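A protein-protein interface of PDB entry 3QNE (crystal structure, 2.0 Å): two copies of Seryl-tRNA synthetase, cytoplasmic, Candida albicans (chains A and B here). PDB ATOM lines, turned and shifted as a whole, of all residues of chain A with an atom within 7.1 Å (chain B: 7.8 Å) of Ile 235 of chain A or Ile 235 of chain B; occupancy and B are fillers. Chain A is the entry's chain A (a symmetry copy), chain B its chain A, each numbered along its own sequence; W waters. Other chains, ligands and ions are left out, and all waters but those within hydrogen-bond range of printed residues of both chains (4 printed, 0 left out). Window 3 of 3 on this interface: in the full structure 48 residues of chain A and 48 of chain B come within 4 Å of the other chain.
N of Ile 235 of chain B sits at hydrogen-bond distance from O of Lys 233 of chain A (2.7 Å). The backbone NH of Gly 237 of chain B lies close to the guanidinium group of Arg 280 of chain A. The guanidinium group of Arg 280 of chain B is in salt-bridge range of the side-chain carboxylate of Asp 236 of chain A, 2.9 Å away. The backbone NH (N) of Gly 237 of chain A lies close to the guanidinium group (NH2) of Arg 280 of chain B, at 3.2 Å. OD1 of Asp 236 of chain B is in salt-bridge range of NE of Arg 280 of chain A. The backbone carbonyl oxygen (O) of Lys 233 of chain B is in hydrogen-bond range of the backbone NH (N) of Ile 235 of chain A, at 2.7 Å.
The backbone NH (N) of Leu 243 of chain B is in hydrogen-bond range of the backbone carbonyl oxygen (O) of Tyr 232 of chain B, at 3.0 Å. The backbone NH of Val 234 of chain A lies within hydrogen-bond range of the backbone carbonyl oxygen of Lys 241 of chain A. O of Lys 241 of chain B is in hydrogen-bond range of N of Val 234 of chain B. The side-chain amino group (NZ) of Lys 233 of chain B lies within hydrogen-bond range of the side-chain hydroxyl (OH) of Tyr 242 of chain B (3.2 Å). NZ of Lys 215 of chain B sits close to NZ of Lys 233 of chain B (2.7 Å).
Among the printed residues, pairs that only touch across the chains: Lys 233 of chain A with Val 234 of chain B (3.4 Å), Val 234 of chain A with Lys 233 of chain B (3.4 Å), Val 234 of chain A with Tyr 232 of chain B (3.4 Å), Tyr 232 of chain A with Val 234 of chain B (3.4 Å), Ile 235 of chain A with Ile 235 of chain B (3.6 Å), Tyr 232 of chain A with Ile 235 of chain B (3.7 Å), Ile 235 of chain A with Tyr 232 of chain B (3.7 Å), Lys 233 of chain A with Lys 233 of chain B (3.8 Å), Tyr 232 of chain A with Asp 236 of chain B (3.8 Å), Asp 236 of chain A with Tyr 232 of chain B (3.8 Å) and Tyr 232 of chain A with Met 212 of chain B (3.9 Å).
Of the printed residues of chain B, Lys 233 of chain A touches Lys 233 (3.8 Å), Val 234 (3.4 Å) and Ile 235 (2.7 Å). Of chain B, only Tyr 232 (3.7 Å), Lys 233 (2.7 Å) and Ile 235 (3.6 Å) come within 4 Å of Ile 235 of chain A. Of the printed residues of chain B, Asp 236 of chain A touches Tyr 232 (3.8 Å) and Arg 280 (2.9 Å). Glu 240 of chain A touches none of the printed residues of chain B. Ile 235 of chain B touches just these residues of chain A: Tyr 232 (3.7 Å), Lys 233 (2.7 Å) and Ile 235 (3.6 Å). Of the printed residues of chain A, Asp 236 of chain B touches Tyr 232 and Arg 280. Of the printed residues of chain A, Gly 237 of chain B touches Arg 280. The nearest residue of chain B that does not touch Ile 235 of chain A is Arg 280 of chain B (4.5 Å). The nearest residue of chain A that does not touch Ile 235 of chain B is Arg 280 of chain A (4.5 Å). The nearest printed residue of chain B that does not touch Gly 237 of chain A is Tyr 232 of chain B (6.3 Å).
Of the 17 printed residues of chain B, 8 touch a printed residue of chain A. Printed residues of chain B that touch a printed residue of chain A: Met 212, Tyr 232, Lys 233, Val 234, Ile 235, Asp 236, Gly 237 and Arg 280. Printed residues of chain A that touch a printed residue of chain B: Tyr 232, Lys 233, Val 234, Ile 235, Asp 236, Gly 237 and Arg 280. Hydrophobic or aromatic side chains of chain A that line the printed part of chain B: Tyr 232, Val 234 and Ile 235. Among the printed residues, Asp or Glu carboxylates within 4 Å of a Lys or Arg side-chain nitrogen of the other chain: Asp 236 of chain A with Arg 280 of chain B (2.9 Å) and Arg 280 of chain A with Asp 236 of chain B (2.9 Å).
Tyr 232 of chain A touches Asp 236 of chain B, and with the chains exchanged Asp 236 of chain A touches Tyr 232 of chain B. Lys 233 of chain B touches its own counterpart, Lys 233 of chain A. Lys 233 of chain A touches Ile 235 of chain B, and with the chains exchanged Ile 235 of chain A touches Lys 233 of chain B. Ile 235 of chain B touches its own counterpart, Ile 235 of chain A. Positions printed for both chains: 231, 232, 233, 234, 235, 236, 237, 238, 239, 240, 241 and 280. Of the 17 pairs that touch across the chains among the printed residues, 16 have their exchanged pair printed and touching as well.
Water W4 lies within hydrogen-bond range of OD2 of Asp 236 of chain B (2.6 Å) and OH of Tyr 232 of chain A (2.7 Å). Water W3 lies within hydrogen-bond range of the side-chain carboxylate (OD2) of Asp 236 of chain A (2.6 Å) and the side-chain hydroxyl (OH) of Tyr 232 of chain B (2.7 Å). Water W2 lies within hydrogen-bond range of the side-chain carboxylate of Asp 236 of chain B (2.9 Å) and the backbone carbonyl oxygen of Arg 280 of chain A (2.9 Å). Water W1 lies within hydrogen-bond range of the side-chain carboxylate of Asp 236 of chain A and the backbone carbonyl oxygen of Arg 280 of chain B.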
ATOM      1  N   LEU A 231      12.370   4.807  -3.452  1.00  0.00           N
ATOM      2  CA  LEU A 231      11.075   4.145  -3.241  1.00  0.00           C
ATOM      3  C   LEU A 231      10.982   3.386  -1.930  1.00  0.00           C
ATOM      4  O   LEU A 231      11.909   2.686  -1.525  1.00  0.00           O
ATOM      5  CB  LEU A 231      10.744   3.187  -4.401  1.00  0.00           C
ATOM      6  CG  LEU A 231      10.847   3.788  -5.802  1.00  0.00           C
ATOM      7  CD1 LEU A 231      10.583   2.738  -6.894  1.00  0.00           C
ATOM      8  CD2 LEU A 231       9.858   4.944  -5.916  1.00  0.00           C
ATOM      9  N   TYR A 232       9.839   3.507  -1.271  1.00  0.00           N
ATOM     10  CA  TYR A 232       9.568   2.676  -0.121  1.00  0.00           C
ATOM     11  C   TYR A 232       9.217   1.284  -0.621  1.00  0.00           C
ATOM     12  O   TYR A 232       8.477   1.135  -1.597  1.00  0.00           O
ATOM     13  CB  TYR A 232       8.365   3.218   0.650  1.00  0.00           C
ATOM     14  CG  TYR A 232       8.595   4.516   1.391  1.00  0.00           C
ATOM     15  CD1 TYR A 232       9.098   4.522   2.688  1.00  0.00           C
ATOM     16  CD2 TYR A 232       8.280   5.733   0.800  1.00  0.00           C
ATOM     17  CE1 TYR A 232       9.285   5.714   3.388  1.00  0.00           C
ATOM     18  CE2 TYR A 232       8.456   6.928   1.481  1.00  0.00           C
ATOM     19  CZ  TYR A 232       8.950   6.916   2.771  1.00  0.00           C
ATOM     20  OH  TYR A 232       9.118   8.121   3.422  1.00  0.00           O
ATOM     21  N   LYS A 233       9.729   0.264   0.048  1.00  0.00           N
ATOM     22  CA  LYS A 233       9.278  -1.093  -0.219  1.00  0.00           C
ATOM     23  C   LYS A 233       8.180  -1.495   0.761  1.00  0.00           C
ATOM     24  O   LYS A 233       8.207  -1.129   1.937  1.00  0.00           O
ATOM     25  CB  LYS A 233      10.443  -2.082  -0.139  1.00  0.00           C
ATOM     26  CG  LYS A 233      11.647  -1.627  -0.906  1.00  0.00           C
ATOM     27  CD  LYS A 233      12.857  -2.479  -0.574  1.00  0.00           C
ATOM     28  CE  LYS A 233      12.604  -3.922  -0.966  1.00  0.00           C
ATOM     29  NZ  LYS A 233      12.259  -3.990  -2.409  1.00  0.00           N
ATOM     30  N   VAL A 234       7.215  -2.251   0.254  1.00  0.00           N
ATOM     31  CA  VAL A 234       6.090  -2.717   1.038  1.00  0.00           C
ATOM     32  C   VAL A 234       6.269  -4.209   1.277  1.00  0.00           C
ATOM     33  O   VAL A 234       6.539  -4.957   0.338  1.00  0.00           O
ATOM     34  CB  VAL A 234       4.787  -2.530   0.232  1.00  0.00           C
ATOM     35  CG1 VAL A 234       3.604  -2.980   1.035  1.00  0.00           C
ATOM     36  CG2 VAL A 234       4.640  -1.068  -0.192  1.00  0.00           C
ATOM     37  N   ILE A 235       6.110  -4.636   2.522  1.00  0.00           N
ATOM     38  CA  ILE A 235       6.187  -6.053   2.876  1.00  0.00           C
ATOM     39  C   ILE A 235       4.790  -6.608   3.065  1.00  0.00           C
ATOM     40  O   ILE A 235       4.012  -6.117   3.891  1.00  0.00           O
ATOM     41  CB  ILE A 235       6.944  -6.288   4.184  1.00  0.00           C
ATOM     42  CG1 ILE A 235       8.326  -5.648   4.121  1.00  0.00           C
ATOM     43  CG2 ILE A 235       7.047  -7.780   4.465  1.00  0.00           C
ATOM     44  CD1 ILE A 235       9.087  -6.017   2.887  1.00  0.00           C
ATOM     45  N   ASP A 236       4.485  -7.642   2.300  1.00  0.00           N
ATOM     46  CA  ASP A 236       3.174  -8.256   2.313  1.00  0.00           C
ATOM     47  C   ASP A 236       3.398  -9.737   2.576  1.00  0.00           C
ATOM     48  O   ASP A 236       3.507 -10.527   1.647  1.00  0.00           O
ATOM     49  CB  ASP A 236       2.519  -8.031   0.959  1.00  0.00           C
ATOM     50  CG  ASP A 236       1.218  -8.784   0.795  1.00  0.00           C
ATOM     51  OD1 ASP A 236       0.702  -9.367   1.778  1.00  0.00           O
ATOM     52  OD2 ASP A 236       0.712  -8.783  -0.347  1.00  0.00           O
ATOM     53  N   GLY A 237       3.489 -10.095   3.853  1.00  0.00           N
ATOM     54  CA  GLY A 237       3.892 -11.433   4.242  1.00  0.00           C
ATOM     55  C   GLY A 237       5.248 -11.781   3.651  1.00  0.00           C
ATOM     56  O   GLY A 237       6.279 -11.259   4.083  1.00  0.00           O
ATOM     57  N   GLU A 238       5.239 -12.655   2.649  1.00  0.00           N
ATOM     58  CA  GLU A 238       6.467 -13.116   2.017  1.00  0.00           C
ATOM     59  C   GLU A 238       6.790 -12.321   0.759  1.00  0.00           C
ATOM     60  O   GLU A 238       7.895 -12.408   0.235  1.00  0.00           O
ATOM     61  CB  GLU A 238       6.366 -14.607   1.674  1.00  0.00           C
ATOM     62  CG  GLU A 238       5.980 -15.504   2.852  1.00  0.00           C
ATOM     63  CD  GLU A 238       7.016 -15.502   3.967  1.00  0.00           C
ATOM     64  OE1 GLU A 238       8.195 -15.191   3.694  1.00  0.00           O
ATOM     65  OE2 GLU A 238       6.649 -15.810   5.123  1.00  0.00           O
ATOM     66  N   ASP A 239       5.824 -11.549   0.278  1.00  0.00           N
ATOM     67  CA  ASP A 239       5.998 -10.808  -0.968  1.00  0.00           C
ATOM     68  C   ASP A 239       6.393  -9.355  -0.718  1.00  0.00           C
ATOM     69  O   ASP A 239       6.319  -8.860   0.409  1.00  0.00           O
ATOM     70  CB  ASP A 239       4.720 -10.864  -1.805  1.00  0.00           C
ATOM     71  CG  ASP A 239       4.279 -12.284  -2.090  1.00  0.00           C
ATOM     72  OD1 ASP A 239       4.953 -12.954  -2.902  1.00  0.00           O
ATOM     73  OD2 ASP A 239       3.267 -12.731  -1.505  1.00  0.00           O
ATOM     74  N   GLU A 240       6.819  -8.683  -1.780  1.00  0.00           N
ATOM     75  CA  GLU A 240       7.218  -7.281  -1.695  1.00  0.00           C
ATOM     76  C   GLU A 240       6.709  -6.512  -2.910  1.00  0.00           C
ATOM     77  O   GLU A 240       6.665  -7.040  -4.023  1.00  0.00           O
ATOM     78  CB  GLU A 240       8.742  -7.152  -1.636  1.00  0.00           C
ATOM     79  CG  GLU A 240       9.400  -7.744  -0.406  1.00  0.00           C
ATOM     80  CD  GLU A 240      10.890  -7.980  -0.610  1.00  0.00           C
ATOM     81  OE1 GLU A 240      11.341  -7.941  -1.776  1.00  0.00           O
ATOM     82  OE2 GLU A 240      11.606  -8.210   0.390  1.00  0.00           O
ATOM     83  N   LYS A 241       6.329  -5.261  -2.683  1.00  0.00           N
ATOM     84  CA  LYS A 241       5.959  -4.352  -3.761  1.00  0.00           C
ATOM     85  C   LYS A 241       6.659  -3.027  -3.455  1.00  0.00           C
ATOM     86  O   LYS A 241       7.357  -2.902  -2.436  1.00  0.00           O
ATOM     87  CB  LYS A 241       4.432  -4.174  -3.838  1.00  0.00           C
ATOM     88  CG  LYS A 241       3.639  -5.483  -3.926  1.00  0.00           C
ATOM     89  CD  LYS A 241       2.169  -5.247  -4.237  1.00  0.00           C
ATOM     90  CE  LYS A 241       1.347  -6.548  -4.197  1.00  0.00           C
ATOM     91  NZ  LYS A 241       1.543  -7.477  -5.373  1.00  0.00           N
ATOM     92  N   ARG A 280      11.144   8.519  -0.326  1.00  0.00           N
ATOM     93  CA  ARG A 280      12.029   8.364   0.830  1.00  0.00           C
ATOM     94  C   ARG A 280      12.881   9.615   1.052  1.00  0.00           C
ATOM     95  O   ARG A 280      13.265   9.922   2.172  1.00  0.00           O
ATOM     96  CB  ARG A 280      12.933   7.134   0.679  1.00  0.00           C
ATOM     97  CG  ARG A 280      12.212   5.788   0.807  1.00  0.00           C
ATOM     98  CD  ARG A 280      13.209   4.640   0.826  1.00  0.00           C
ATOM     99  NE  ARG A 280      14.206   4.837   1.873  1.00  0.00           N
ATOM    100  CZ  ARG A 280      15.475   4.448   1.788  1.00  0.00           C
ATOM    101  NH1 ARG A 280      15.903   3.831   0.698  1.00  0.00           N
ATOM    102  NH2 ARG A 280      16.313   4.682   2.798  1.00  0.00           N
ATOM    103  N   MET B 212       1.110   6.458   6.778  1.00  0.00           N
ATOM    104  CA  MET B 212       2.150   5.683   7.439  1.00  0.00           C
ATOM    105  C   MET B 212       2.151   6.043   8.912  1.00  0.00           C
ATOM    106  O   MET B 212       1.866   7.182   9.277  1.00  0.00           O
ATOM    107  CB  MET B 212       3.522   5.989   6.857  1.00  0.00           C
ATOM    108  CG  MET B 212       3.698   5.524   5.430  1.00  0.00           C
ATOM    109  SD  MET B 212       5.376   5.793   4.892  1.00  0.00           S
ATOM    110  CE  MET B 212       5.224   5.320   3.172  1.00  0.00           C
ATOM    111  N   LYS B 215       5.692   2.256  14.300  1.00  0.00           N
ATOM    112  CA  LYS B 215       5.261   1.011  14.928  1.00  0.00           C
ATOM    113  C   LYS B 215       4.812   1.181  16.376  1.00  0.00           C
ATOM    114  O   LYS B 215       3.790   0.643  16.788  1.00  0.00           O
ATOM    115  CB  LYS B 215       6.389  -0.008  14.873  1.00  0.00           C
ATOM    116  CG  LYS B 215       6.641  -0.578  13.490  1.00  0.00           C
ATOM    117  CD  LYS B 215       7.701  -1.657  13.570  1.00  0.00           C
ATOM    118  CE  LYS B 215       7.639  -2.573  12.373  1.00  0.00           C
ATOM    119  NZ  LYS B 215       8.507  -3.771  12.562  1.00  0.00           N
ATOM    120  N   PHE B 227      -1.250  -6.559  13.326  1.00  0.00           N
ATOM    121  CA  PHE B 227       0.078  -6.508  12.736  1.00  0.00           C
ATOM    122  C   PHE B 227       0.402  -7.742  11.901  1.00  0.00           C
ATOM    123  O   PHE B 227       0.710  -7.640  10.710  1.00  0.00           O
ATOM    124  CB  PHE B 227       1.127  -6.328  13.821  1.00  0.00           C
ATOM    125  CG  PHE B 227       0.997  -5.033  14.571  1.00  0.00           C
ATOM    126  CD1 PHE B 227       1.726  -3.922  14.185  1.00  0.00           C
ATOM    127  CD2 PHE B 227       0.140  -4.927  15.657  1.00  0.00           C
ATOM    128  CE1 PHE B 227       1.609  -2.725  14.872  1.00  0.00           C
ATOM    129  CE2 PHE B 227       0.021  -3.742  16.349  1.00  0.00           C
ATOM    130  CZ  PHE B 227       0.752  -2.637  15.955  1.00  0.00           C
ATOM    131  N   LEU B 231      -1.756  -5.515   8.482  1.00  0.00           N
ATOM    132  CA  LEU B 231      -1.057  -4.298   8.044  1.00  0.00           C
ATOM    133  C   LEU B 231       0.142  -4.567   7.152  1.00  0.00           C
ATOM    134  O   LEU B 231       0.938  -5.470   7.401  1.00  0.00           O
ATOM    135  CB  LEU B 231      -0.606  -3.451   9.249  1.00  0.00           C
ATOM    136  CG  LEU B 231      -1.693  -3.138  10.277  1.00  0.00           C
ATOM    137  CD1 LEU B 231      -1.131  -2.365  11.482  1.00  0.00           C
ATOM    138  CD2 LEU B 231      -2.802  -2.342   9.596  1.00  0.00           C
ATOM    139  N   TYR B 232       0.283  -3.757   6.114  1.00  0.00           N
ATOM    140  CA  TYR B 232       1.488  -3.795   5.318  1.00  0.00           C
ATOM    141  C   TYR B 232       2.590  -3.101   6.103  1.00  0.00           C
ATOM    142  O   TYR B 232       2.362  -2.052   6.712  1.00  0.00           O
ATOM    143  CB  TYR B 232       1.283  -3.027   4.012  1.00  0.00           C
ATOM    144  CG  TYR B 232       0.360  -3.680   3.009  1.00  0.00           C
ATOM    145  CD1 TYR B 232       0.842  -4.603   2.085  1.00  0.00           C
ATOM    146  CD2 TYR B 232      -0.988  -3.350   2.969  1.00  0.00           C
ATOM    147  CE1 TYR B 232       0.002  -5.187   1.138  1.00  0.00           C
ATOM    148  CE2 TYR B 232      -1.839  -3.918   2.032  1.00  0.00           C
ATOM    149  CZ  TYR B 232      -1.343  -4.827   1.117  1.00  0.00           C
ATOM    150  OH  TYR B 232      -2.214  -5.379   0.200  1.00  0.00           O
ATOM    151  N   LYS B 233       3.785  -3.668   6.081  1.00  0.00           N
ATOM    152  CA  LYS B 233       4.942  -2.967   6.616  1.00  0.00           C
ATOM    153  C   LYS B 233       5.690  -2.240   5.503  1.00  0.00           C
ATOM    154  O   LYS B 233       5.794  -2.728   4.378  1.00  0.00           O
ATOM    155  CB  LYS B 233       5.883  -3.937   7.334  1.00  0.00           C
ATOM    156  CG  LYS B 233       5.167  -4.846   8.286  1.00  0.00           C
ATOM    157  CD  LYS B 233       6.076  -5.965   8.759  1.00  0.00           C
ATOM    158  CE  LYS B 233       7.265  -5.392   9.505  1.00  0.00           C
ATOM    159  NZ  LYS B 233       6.785  -4.556  10.635  1.00  0.00           N
ATOM    160  N   VAL B 234       6.202  -1.062   5.838  1.00  0.00           N
ATOM    161  CA  VAL B 234       6.935  -0.232   4.905  1.00  0.00           C
ATOM    162  C   VAL B 234       8.406  -0.274   5.293  1.00  0.00           C
ATOM    163  O   VAL B 234       8.741  -0.090   6.462  1.00  0.00           O
ATOM    164  CB  VAL B 234       6.462   1.232   5.038  1.00  0.00           C
ATOM    165  CG1 VAL B 234       7.187   2.108   4.062  1.00  0.00           C
ATOM    166  CG2 VAL B 234       4.949   1.314   4.833  1.00  0.00           C
ATOM    167  N   ILE B 235       9.272  -0.505   4.315  1.00  0.00           N
ATOM    168  CA  ILE B 235      10.718  -0.504   4.539  1.00  0.00           C
ATOM    169  C   ILE B 235      11.308   0.801   4.044  1.00  0.00           C
ATOM    170  O   ILE B 235      11.169   1.163   2.870  1.00  0.00           O
ATOM    171  CB  ILE B 235      11.425  -1.631   3.787  1.00  0.00           C
ATOM    172  CG1 ILE B 235      10.803  -2.977   4.137  1.00  0.00           C
ATOM    173  CG2 ILE B 235      12.912  -1.617   4.109  1.00  0.00           C
ATOM    174  CD1 ILE B 235      10.676  -3.198   5.612  1.00  0.00           C
ATOM    175  N   ASP B 236      11.979   1.495   4.948  1.00  0.00           N
ATOM    176  CA  ASP B 236      12.557   2.790   4.658  1.00  0.00           C
ATOM    177  C   ASP B 236      14.027   2.696   5.036  1.00  0.00           C
ATOM    178  O   ASP B 236      14.407   3.031   6.150  1.00  0.00           O
ATOM    179  CB  ASP B 236      11.840   3.842   5.491  1.00  0.00           C
ATOM    180  CG  ASP B 236      12.481   5.208   5.405  1.00  0.00           C
ATOM    181  OD1 ASP B 236      13.394   5.421   4.572  1.00  0.00           O
ATOM    182  OD2 ASP B 236      12.051   6.077   6.192  1.00  0.00           O
ATOM    183  N   GLY B 237      14.840   2.214   4.102  1.00  0.00           N
ATOM    184  CA  GLY B 237      16.224   1.889   4.391  1.00  0.00           C
ATOM    185  C   GLY B 237      16.317   0.890   5.531  1.00  0.00           C
ATOM    186  O   GLY B 237      15.993  -0.289   5.367  1.00  0.00           O
ATOM    187  N   GLU B 238      16.748   1.372   6.694  1.00  0.00           N
ATOM    188  CA  GLU B 238      16.932   0.520   7.861  1.00  0.00           C
ATOM    189  C   GLU B 238      15.719   0.552   8.782  1.00  0.00           C
ATOM    190  O   GLU B 238      15.596  -0.274   9.679  1.00  0.00           O
ATOM    191  CB  GLU B 238      18.183   0.942   8.641  1.00  0.00           C
ATOM    192  CG  GLU B 238      19.459   1.010   7.801  1.00  0.00           C
ATOM    193  CD  GLU B 238      19.875  -0.341   7.235  1.00  0.00           C
ATOM    194  OE1 GLU B 238      19.479  -1.380   7.806  1.00  0.00           O
ATOM    195  OE2 GLU B 238      20.598  -0.364   6.215  1.00  0.00           O
ATOM    196  N   ASP B 239      14.826   1.509   8.558  1.00  0.00           N
ATOM    197  CA  ASP B 239      13.669   1.682   9.430  1.00  0.00           C
ATOM    198  C   ASP B 239      12.416   1.027   8.856  1.00  0.00           C
ATOM    199  O   ASP B 239      12.383   0.631   7.688  1.00  0.00           O
ATOM    200  CB  ASP B 239      13.410   3.168   9.685  1.00  0.00           C
ATOM    201  CG  ASP B 239      14.619   3.873  10.262  1.00  0.00           C
ATOM    202  OD1 ASP B 239      14.929   3.628  11.447  1.00  0.00           O
ATOM    203  OD2 ASP B 239      15.259   4.667   9.534  1.00  0.00           O
ATOM    204  N   GLU B 240      11.391   0.912   9.690  1.00  0.00           N
ATOM    205  CA  GLU B 240      10.124   0.318   9.276  1.00  0.00           C
ATOM    206  C   GLU B 240       8.955   1.109   9.854  1.00  0.00           C
ATOM    207  O   GLU B 240       9.023   1.614  10.977  1.00  0.00           O
ATOM    208  CB  GLU B 240      10.020  -1.131   9.755  1.00  0.00           C
ATOM    209  CG  GLU B 240      11.029  -2.090   9.158  1.00  0.00           C
ATOM    210  CD  GLU B 240      11.165  -3.366   9.978  1.00  0.00           C
ATOM    211  OE1 GLU B 240      10.686  -3.379  11.134  1.00  0.00           O
ATOM    212  OE2 GLU B 240      11.753  -4.348   9.472  1.00  0.00           O
ATOM    213  N   LYS B 241       7.884   1.207   9.077  1.00  0.00           N
ATOM    214  CA  LYS B 241       6.636   1.802   9.541  1.00  0.00           C
ATOM    215  C   LYS B 241       5.522   0.863   9.078  1.00  0.00           C
ATOM    216  O   LYS B 241       5.788  -0.159   8.426  1.00  0.00           O
ATOM    217  CB  LYS B 241       6.450   3.219   8.968  1.00  0.00           C
ATOM    218  CG  LYS B 241       7.631   4.165   9.204  1.00  0.00           C
ATOM    219  CD  LYS B 241       7.302   5.603   8.832  1.00  0.00           C
ATOM    220  CE  LYS B 241       8.525   6.531   8.945  1.00  0.00           C
ATOM    221  NZ  LYS B 241       8.940   6.891  10.352  1.00  0.00           N
ATOM    222  N   TYR B 242       4.286   1.171   9.446  1.00  0.00           N
ATOM    223  CA  TYR B 242       3.147   0.429   8.907  1.00  0.00           C
ATOM    224  C   TYR B 242       2.319   1.358   8.038  1.00  0.00           C
ATOM    225  O   TYR B 242       2.274   2.555   8.295  1.00  0.00           O
ATOM    226  CB  TYR B 242       2.257  -0.083  10.036  1.00  0.00           C
ATOM    227  CG  TYR B 242       2.864  -1.216  10.805  1.00  0.00           C
ATOM    228  CD1 TYR B 242       2.880  -2.505  10.284  1.00  0.00           C
ATOM    229  CD2 TYR B 242       3.428  -1.003  12.048  1.00  0.00           C
ATOM    230  CE1 TYR B 242       3.441  -3.546  10.986  1.00  0.00           C
ATOM    231  CE2 TYR B 242       3.987  -2.036  12.756  1.00  0.00           C
ATOM    232  CZ  TYR B 242       3.998  -3.304  12.224  1.00  0.00           C
ATOM    233  OH  TYR B 242       4.560  -4.334  12.943  1.00  0.00           O
ATOM    234  N   LEU B 243       1.644   0.802   7.032  1.00  0.00           N
ATOM    235  CA  LEU B 243       0.586   1.521   6.357  1.00  0.00           C
ATOM    236  C   LEU B 243      -0.674   1.326   7.178  1.00  0.00           C
ATOM    237  O   LEU B 243      -0.919   0.237   7.705  1.00  0.00           O
ATOM    238  CB  LEU B 243       0.381   0.964   4.943  1.00  0.00           C
ATOM    239  CG  LEU B 243       1.459   1.311   3.914  1.00  0.00           C
ATOM    240  CD1 LEU B 243       1.151   0.615   2.586  1.00  0.00           C
ATOM    241  CD2 LEU B 243       1.496   2.805   3.706  1.00  0.00           C
ATOM    242  N   ARG B 280      -4.006  -5.994   4.036  1.00  0.00           N
ATOM    243  CA  ARG B 280      -3.430  -7.198   3.434  1.00  0.00           C
ATOM    244  C   ARG B 280      -4.508  -8.238   3.127  1.00  0.00           C
ATOM    245  O   ARG B 280      -4.371  -9.030   2.205  1.00  0.00           O
ATOM    246  CB  ARG B 280      -2.352  -7.810   4.338  1.00  0.00           C
ATOM    247  CG  ARG B 280      -1.054  -7.001   4.428  1.00  0.00           C
ATOM    248  CD  ARG B 280       0.012  -7.772   5.192  1.00  0.00           C
ATOM    249  NE  ARG B 280       0.220  -9.089   4.602  1.00  0.00           N
ATOM    250  CZ  ARG B 280       0.543 -10.180   5.290  1.00  0.00           C
ATOM    251  NH1 ARG B 280       0.701 -10.108   6.603  1.00  0.00           N
ATOM    252  NH2 ARG B 280       0.704 -11.343   4.660  1.00  0.00           N
HETATM  253  O   HOH W   1      -1.981 -10.040   0.852  1.00  0.00           O
HETATM  254  O   HOH W   2      13.680   8.324   4.589  1.00  0.00           O
HETATM  255  O   HOH W   3      -1.156  -7.257  -1.354  1.00  0.00           O
HETATM  256  O   HOH W   4      10.266   7.948   5.812  1.00  0.00           O
